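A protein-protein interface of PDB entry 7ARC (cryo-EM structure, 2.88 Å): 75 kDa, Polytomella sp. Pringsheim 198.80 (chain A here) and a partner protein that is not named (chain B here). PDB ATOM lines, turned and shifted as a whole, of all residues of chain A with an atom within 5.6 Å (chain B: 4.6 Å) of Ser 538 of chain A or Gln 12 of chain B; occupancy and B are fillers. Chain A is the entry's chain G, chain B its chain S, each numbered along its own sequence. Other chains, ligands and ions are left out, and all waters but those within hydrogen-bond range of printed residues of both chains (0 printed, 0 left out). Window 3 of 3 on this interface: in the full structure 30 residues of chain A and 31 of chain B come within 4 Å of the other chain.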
ATOM      1  N   ASN A 347      15.700  18.238  18.666  1.00  0.00           N
ATOM      2  CA  ASN A 347      15.882  18.954  19.924  1.00  0.00           C
ATOM      3  C   ASN A 347      14.585  19.507  20.489  1.00  0.00           C
ATOM      4  O   ASN A 347      14.604  20.079  21.584  1.00  0.00           O
ATOM      5  CB  ASN A 347      16.895  20.085  19.745  1.00  0.00           C
ATOM      6  CG  ASN A 347      18.322  19.582  19.672  1.00  0.00           C
ATOM      7  OD1 ASN A 347      18.593  18.410  19.934  1.00  0.00           O
ATOM      8  ND2 ASN A 347      19.244  20.467  19.314  1.00  0.00           N
ATOM      9  N   GLY A 375      19.320  15.739  21.985  1.00  0.00           N
ATOM     10  CA  GLY A 375      20.442  15.891  22.888  1.00  0.00           C
ATOM     11  C   GLY A 375      20.160  16.900  23.980  1.00  0.00           C
ATOM     12  O   GLY A 375      21.060  17.291  24.727  1.00  0.00           O
ATOM     13  N   ASN A 376      18.903  17.333  24.078  1.00  0.00           N
ATOM     14  CA  ASN A 376      18.485  18.338  25.055  1.00  0.00           C
ATOM     15  C   ASN A 376      18.181  17.660  26.393  1.00  0.00           C
ATOM     16  O   ASN A 376      17.039  17.565  26.845  1.00  0.00           O
ATOM     17  CB  ASN A 376      17.286  19.115  24.530  1.00  0.00           C
ATOM     18  CG  ASN A 376      17.334  20.581  24.903  1.00  0.00           C
ATOM     19  OD1 ASN A 376      18.163  21.004  25.708  1.00  0.00           O
ATOM     20  ND2 ASN A 376      16.443  21.368  24.317  1.00  0.00           N
ATOM     21  N   LEU A 377      19.244  17.178  27.031  1.00  0.00           N
ATOM     22  CA  LEU A 377      19.166  16.478  28.310  1.00  0.00           C
ATOM     23  C   LEU A 377      19.798  17.369  29.371  1.00  0.00           C
ATOM     24  O   LEU A 377      21.014  17.573  29.365  1.00  0.00           O
ATOM     25  CB  LEU A 377      19.882  15.132  28.236  1.00  0.00           C
ATOM     26  CG  LEU A 377      19.460  14.160  27.135  1.00  0.00           C
ATOM     27  CD1 LEU A 377      20.493  13.062  26.980  1.00  0.00           C
ATOM     28  CD2 LEU A 377      18.100  13.568  27.422  1.00  0.00           C
ATOM     29  N   VAL A 536      24.238  15.259  29.719  1.00  0.00           N
ATOM     30  CA  VAL A 536      24.630  16.651  29.506  1.00  0.00           C
ATOM     31  C   VAL A 536      24.099  17.104  28.149  1.00  0.00           C
ATOM     32  O   VAL A 536      24.009  16.285  27.223  1.00  0.00           O
ATOM     33  CB  VAL A 536      26.162  16.792  29.608  1.00  0.00           C
ATOM     34  CG1 VAL A 536      26.852  15.866  28.618  1.00  0.00           C
ATOM     35  CG2 VAL A 536      26.624  18.224  29.407  1.00  0.00           C
ATOM     36  N   PRO A 537      23.711  18.372  27.985  1.00  0.00           N
ATOM     37  CA  PRO A 537      23.281  18.843  26.663  1.00  0.00           C
ATOM     38  C   PRO A 537      24.362  18.662  25.608  1.00  0.00           C
ATOM     39  O   PRO A 537      25.549  18.880  25.859  1.00  0.00           O
ATOM     40  CB  PRO A 537      22.983  20.325  26.903  1.00  0.00           C
ATOM     41  CG  PRO A 537      22.597  20.384  28.320  1.00  0.00           C
ATOM     42  CD  PRO A 537      23.489  19.400  29.016  1.00  0.00           C
ATOM     43  N   SER A 538      23.934  18.259  24.417  1.00  0.00           N
ATOM     44  CA  SER A 538      24.852  18.023  23.317  1.00  0.00           C
ATOM     45  C   SER A 538      25.284  19.348  22.697  1.00  0.00           C
ATOM     46  O   SER A 538      24.805  20.424  23.064  1.00  0.00           O
ATOM     47  CB  SER A 538      24.206  17.127  22.264  1.00  0.00           C
ATOM     48  OG  SER A 538      23.320  17.865  21.442  1.00  0.00           O
ATOM     49  N   ALA A 539      26.216  19.259  21.748  1.00  0.00           N
ATOM     50  CA  ALA A 539      26.725  20.458  21.092  1.00  0.00           C
ATOM     51  C   ALA A 539      25.623  21.201  20.349  1.00  0.00           C
ATOM     52  O   ALA A 539      25.550  22.433  20.404  1.00  0.00           O
ATOM     53  CB  ALA A 539      27.861  20.093  20.137  1.00  0.00           C
ATOM     54  N   SER A 540      24.756  20.467  19.646  1.00  0.00           N
ATOM     55  CA  SER A 540      23.689  21.103  18.879  1.00  0.00           C
ATOM     56  C   SER A 540      22.705  21.836  19.783  1.00  0.00           C
ATOM     57  O   SER A 540      22.261  22.943  19.458  1.00  0.00           O
ATOM     58  CB  SER A 540      22.962  20.060  18.033  1.00  0.00           C
ATOM     59  OG  SER A 540      23.827  19.496  17.065  1.00  0.00           O
ATOM     60  N   ALA A 541      22.345  21.231  20.917  1.00  0.00           N
ATOM     61  CA  ALA A 541      21.359  21.847  21.800  1.00  0.00           C
ATOM     62  C   ALA A 541      21.857  23.181  22.337  1.00  0.00           C
ATOM     63  O   ALA A 541      21.100  24.157  22.398  1.00  0.00           O
ATOM     64  CB  ALA A 541      21.020  20.899  22.950  1.00  0.00           C
ATOM     65  N   ARG A 542      23.124  23.240  22.748  1.00  0.00           N
ATOM     66  CA  ARG A 542      23.690  24.494  23.234  1.00  0.00           C
ATOM     67  C   ARG A 542      23.897  25.490  22.098  1.00  0.00           C
ATOM     68  O   ARG A 542      23.646  26.688  22.267  1.00  0.00           O
ATOM     69  CB  ARG A 542      25.000  24.227  23.971  1.00  0.00           C
ATOM     70  CG  ARG A 542      24.918  23.062  24.939  1.00  0.00           C
ATOM     71  CD  ARG A 542      26.288  22.641  25.429  1.00  0.00           C
ATOM     72  NE  ARG A 542      26.945  23.713  26.165  1.00  0.00           N
ATOM     73  CZ  ARG A 542      28.153  23.624  26.700  1.00  0.00           C
ATOM     74  NH1 ARG A 542      28.878  22.524  26.591  1.00  0.00           N
ATOM     75  NH2 ARG A 542      28.649  24.667  27.358  1.00  0.00           N
ATOM     76  N   THR A 543      24.370  25.019  20.941  1.00  0.00           N
ATOM     77  CA  THR A 543      24.655  25.922  19.829  1.00  0.00           C
ATOM     78  C   THR A 543      23.388  26.603  19.326  1.00  0.00           C
ATOM     79  O   THR A 543      23.355  27.827  19.150  1.00  0.00           O
ATOM     80  CB  THR A 543      25.332  25.158  18.690  1.00  0.00           C
ATOM     81  OG1 THR A 543      26.675  24.831  19.059  1.00  0.00           O
ATOM     82  CG2 THR A 543      25.351  25.999  17.420  1.00  0.00           C
ATOM     83  N   THR B  10      30.704  15.498  13.506  1.00  0.00           N
ATOM     84  CA  THR B  10      30.539  14.052  13.382  1.00  0.00           C
ATOM     85  C   THR B  10      29.999  13.407  14.655  1.00  0.00           C
ATOM     86  O   THR B  10      28.935  12.782  14.633  1.00  0.00           O
ATOM     87  CB  THR B  10      31.873  13.407  12.989  1.00  0.00           C
ATOM     88  OG1 THR B  10      32.408  14.077  11.842  1.00  0.00           O
ATOM     89  CG2 THR B  10      31.676  11.938  12.666  1.00  0.00           C
ATOM     90  N   PHE B  11      30.712  13.547  15.767  1.00  0.00           N
ATOM     91  CA  PHE B  11      30.334  12.856  16.989  1.00  0.00           C
ATOM     92  C   PHE B  11      29.327  13.666  17.789  1.00  0.00           C
ATOM     93  O   PHE B  11      29.452  14.887  17.924  1.00  0.00           O
ATOM     94  CB  PHE B  11      31.551  12.575  17.873  1.00  0.00           C
ATOM     95  CG  PHE B  11      32.613  11.753  17.215  1.00  0.00           C
ATOM     96  CD1 PHE B  11      32.282  10.755  16.320  1.00  0.00           C
ATOM     97  CD2 PHE B  11      33.946  11.961  17.515  1.00  0.00           C
ATOM     98  CE1 PHE B  11      33.263   9.993  15.724  1.00  0.00           C
ATOM     99  CE2 PHE B  11      34.928  11.201  16.922  1.00  0.00           C
ATOM    100  CZ  PHE B  11      34.586  10.215  16.028  1.00  0.00           C
ATOM    101  N   GLN B  12      28.324  12.969  18.314  1.00  0.00           N
ATOM    102  CA  GLN B  12      27.462  13.548  19.333  1.00  0.00           C
ATOM    103  C   GLN B  12      28.132  13.500  20.696  1.00  0.00           C
ATOM    104  O   GLN B  12      27.988  14.431  21.497  1.00  0.00           O
ATOM    105  CB  GLN B  12      26.121  12.816  19.373  1.00  0.00           C
ATOM    106  CG  GLN B  12      25.290  12.995  18.123  1.00  0.00           C
ATOM    107  CD  GLN B  12      24.598  14.335  18.087  1.00  0.00           C
ATOM    108  OE1 GLN B  12      24.150  14.842  19.114  1.00  0.00           O
ATOM    109  NE2 GLN B  12      24.508  14.923  16.902  1.00  0.00           N
ATOM    110  N   GLU B  13      28.864  12.426  20.975  1.00  0.00           N
ATOM    111  CA  GLU B  13      29.636  12.338  22.200  1.00  0.00           C
ATOM    112  C   GLU B  13      30.805  11.391  21.979  1.00  0.00           C
ATOM    113  O   GLU B  13      30.764  10.521  21.106  1.00  0.00           O
ATOM    114  CB  GLU B  13      28.719  11.863  23.327  1.00  0.00           C
ATOM    115  CG  GLU B  13      29.288  11.778  24.705  1.00  0.00           C
ATOM    116  CD  GLU B  13      28.219  11.343  25.678  1.00  0.00           C
ATOM    117  OE1 GLU B  13      27.085  11.085  25.228  1.00  0.00           O
ATOM    118  OE2 GLU B  13      28.481  11.293  26.887  1.00  0.00           O
ATOM    119  N   LEU B  46      31.810  19.804  22.277  1.00  0.00           N
ATOM    120  CA  LEU B  46      31.701  18.351  22.223  1.00  0.00           C
ATOM    121  C   LEU B  46      31.986  17.747  23.595  1.00  0.00           C
ATOM    122  O   LEU B  46      33.007  18.075  24.208  1.00  0.00           O
ATOM    123  CB  LEU B  46      32.672  17.789  21.189  1.00  0.00           C
ATOM    124  CG  LEU B  46      32.777  16.267  21.103  1.00  0.00           C
ATOM    125  CD1 LEU B  46      31.541  15.692  20.446  1.00  0.00           C
ATOM    126  CD2 LEU B  46      34.027  15.861  20.349  1.00  0.00           C
ATOM    127  N   PRO B  47      31.117  16.875  24.111  1.00  0.00           N
ATOM    128  CA  PRO B  47      31.414  16.156  25.358  1.00  0.00           C
ATOM    129  C   PRO B  47      32.380  15.006  25.116  1.00  0.00           C
ATOM    130  O   PRO B  47      32.020  13.987  24.520  1.00  0.00           O
ATOM    131  CB  PRO B  47      30.030  15.658  25.805  1.00  0.00           C
ATOM    132  CG  PRO B  47      29.039  16.426  24.946  1.00  0.00           C
ATOM    133  CD  PRO B  47      29.752  16.587  23.654  1.00  0.00           C
ATOM    134  N   ARG B  63      29.604   8.068  19.908  1.00  0.00           N
ATOM    135  CA  ARG B  63      28.168   7.992  19.674  1.00  0.00           C
ATOM    136  C   ARG B  63      27.794   8.941  18.542  1.00  0.00           C
ATOM    137  O   ARG B  63      28.043  10.147  18.629  1.00  0.00           O
ATOM    138  CB  ARG B  63      27.384   8.316  20.944  1.00  0.00           C
ATOM    139  CG  ARG B  63      25.904   8.013  20.821  1.00  0.00           C
ATOM    140  CD  ARG B  63      25.121   8.485  22.027  1.00  0.00           C
ATOM    141  NE  ARG B  63      24.772   9.896  21.942  1.00  0.00           N
ATOM    142  CZ  ARG B  63      24.899  10.753  22.945  1.00  0.00           C
ATOM    143  NH1 ARG B  63      25.307  10.359  24.138  1.00  0.00           N
ATOM    144  NH2 ARG B  63      24.592  12.031  22.751  1.00  0.00           N
ATOM    145  N   TYR B  64      27.203   8.392  17.487  1.00  0.00           N
ATOM    146  CA  TYR B  64      26.733   9.173  16.356  1.00  0.00           C
ATOM    147  C   TYR B  64      25.256   9.511  16.526  1.00  0.00           C
ATOM    148  O   TYR B  64      24.624   9.173  17.529  1.00  0.00           O
ATOM    149  CB  TYR B  64      26.975   8.421  15.050  1.00  0.00           C
ATOM    150  CG  TYR B  64      28.365   7.854  14.929  1.00  0.00           C
ATOM    151  CD1 TYR B  64      29.432   8.661  14.570  1.00  0.00           C
ATOM    152  CD2 TYR B  64      28.611   6.511  15.166  1.00  0.00           C
ATOM    153  CE1 TYR B  64      30.701   8.149  14.456  1.00  0.00           C
ATOM    154  CE2 TYR B  64      29.880   5.991  15.052  1.00  0.00           C
ATOM    155  CZ  TYR B  64      30.920   6.816  14.696  1.00  0.00           C
ATOM    156  OH  TYR B  64      32.191   6.307  14.580  1.00  0.00           O
ATOM    157  N   ASP B  65      24.702  10.207  15.537  1.00  0.00           N
ATOM    158  CA  ASP B  65      23.295  10.577  15.582  1.00  0.00           C
ATOM    159  C   ASP B  65      22.415   9.335  15.626  1.00  0.00           C
ATOM    160  O   ASP B  65      22.744   8.299  15.039  1.00  0.00           O
ATOM    161  CB  ASP B  65      22.938  11.432  14.366  1.00  0.00           C
ATOM    162  CG  ASP B  65      21.805  12.393  14.646  1.00  0.00           C
ATOM    163  OD1 ASP B  65      21.357  12.461  15.809  1.00  0.00           O
ATOM    164  OD2 ASP B  65      21.363  13.084  13.703  1.00  0.00           O
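The backbone NH of Gln 12 of chain B lies within hydrogen-bond range of the backbone carbonyl oxygen of Arg 63 of chain B, at 2.9 Å. The backbone NH (N) of Ser 538 of chain A lies within hydrogen-bond range of the backbone carbonyl oxygen (O) of Gly 375 of chain A, at 3.0 Å. N of Ser 540 of chain A lies close to OG of Ser 538 of chain A (3.5 Å).
Among the printed residues, pairs that only touch across the chains: Ser 538 of chain A with Gln 12 of chain B (3.9 Å).
Of the printed residues of chain B, Ser 538 of chain A touches Gln 12. Of the printed residues of chain A, Gln 12 of chain B touches Ser 538. Pro 537 of chain A touches none of the printed residues of chain B. Gly 375 of chain A touches none of the printed residues of chain B. The nearest residue of chain A that does not touch Gln 12 of chain B is Ser 540 of chain A (4.6 Å).
Among the printed residues, no Asp or Glu carboxylate lies within 4 Å of a Lys or Arg side-chain nitrogen of the other chain.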
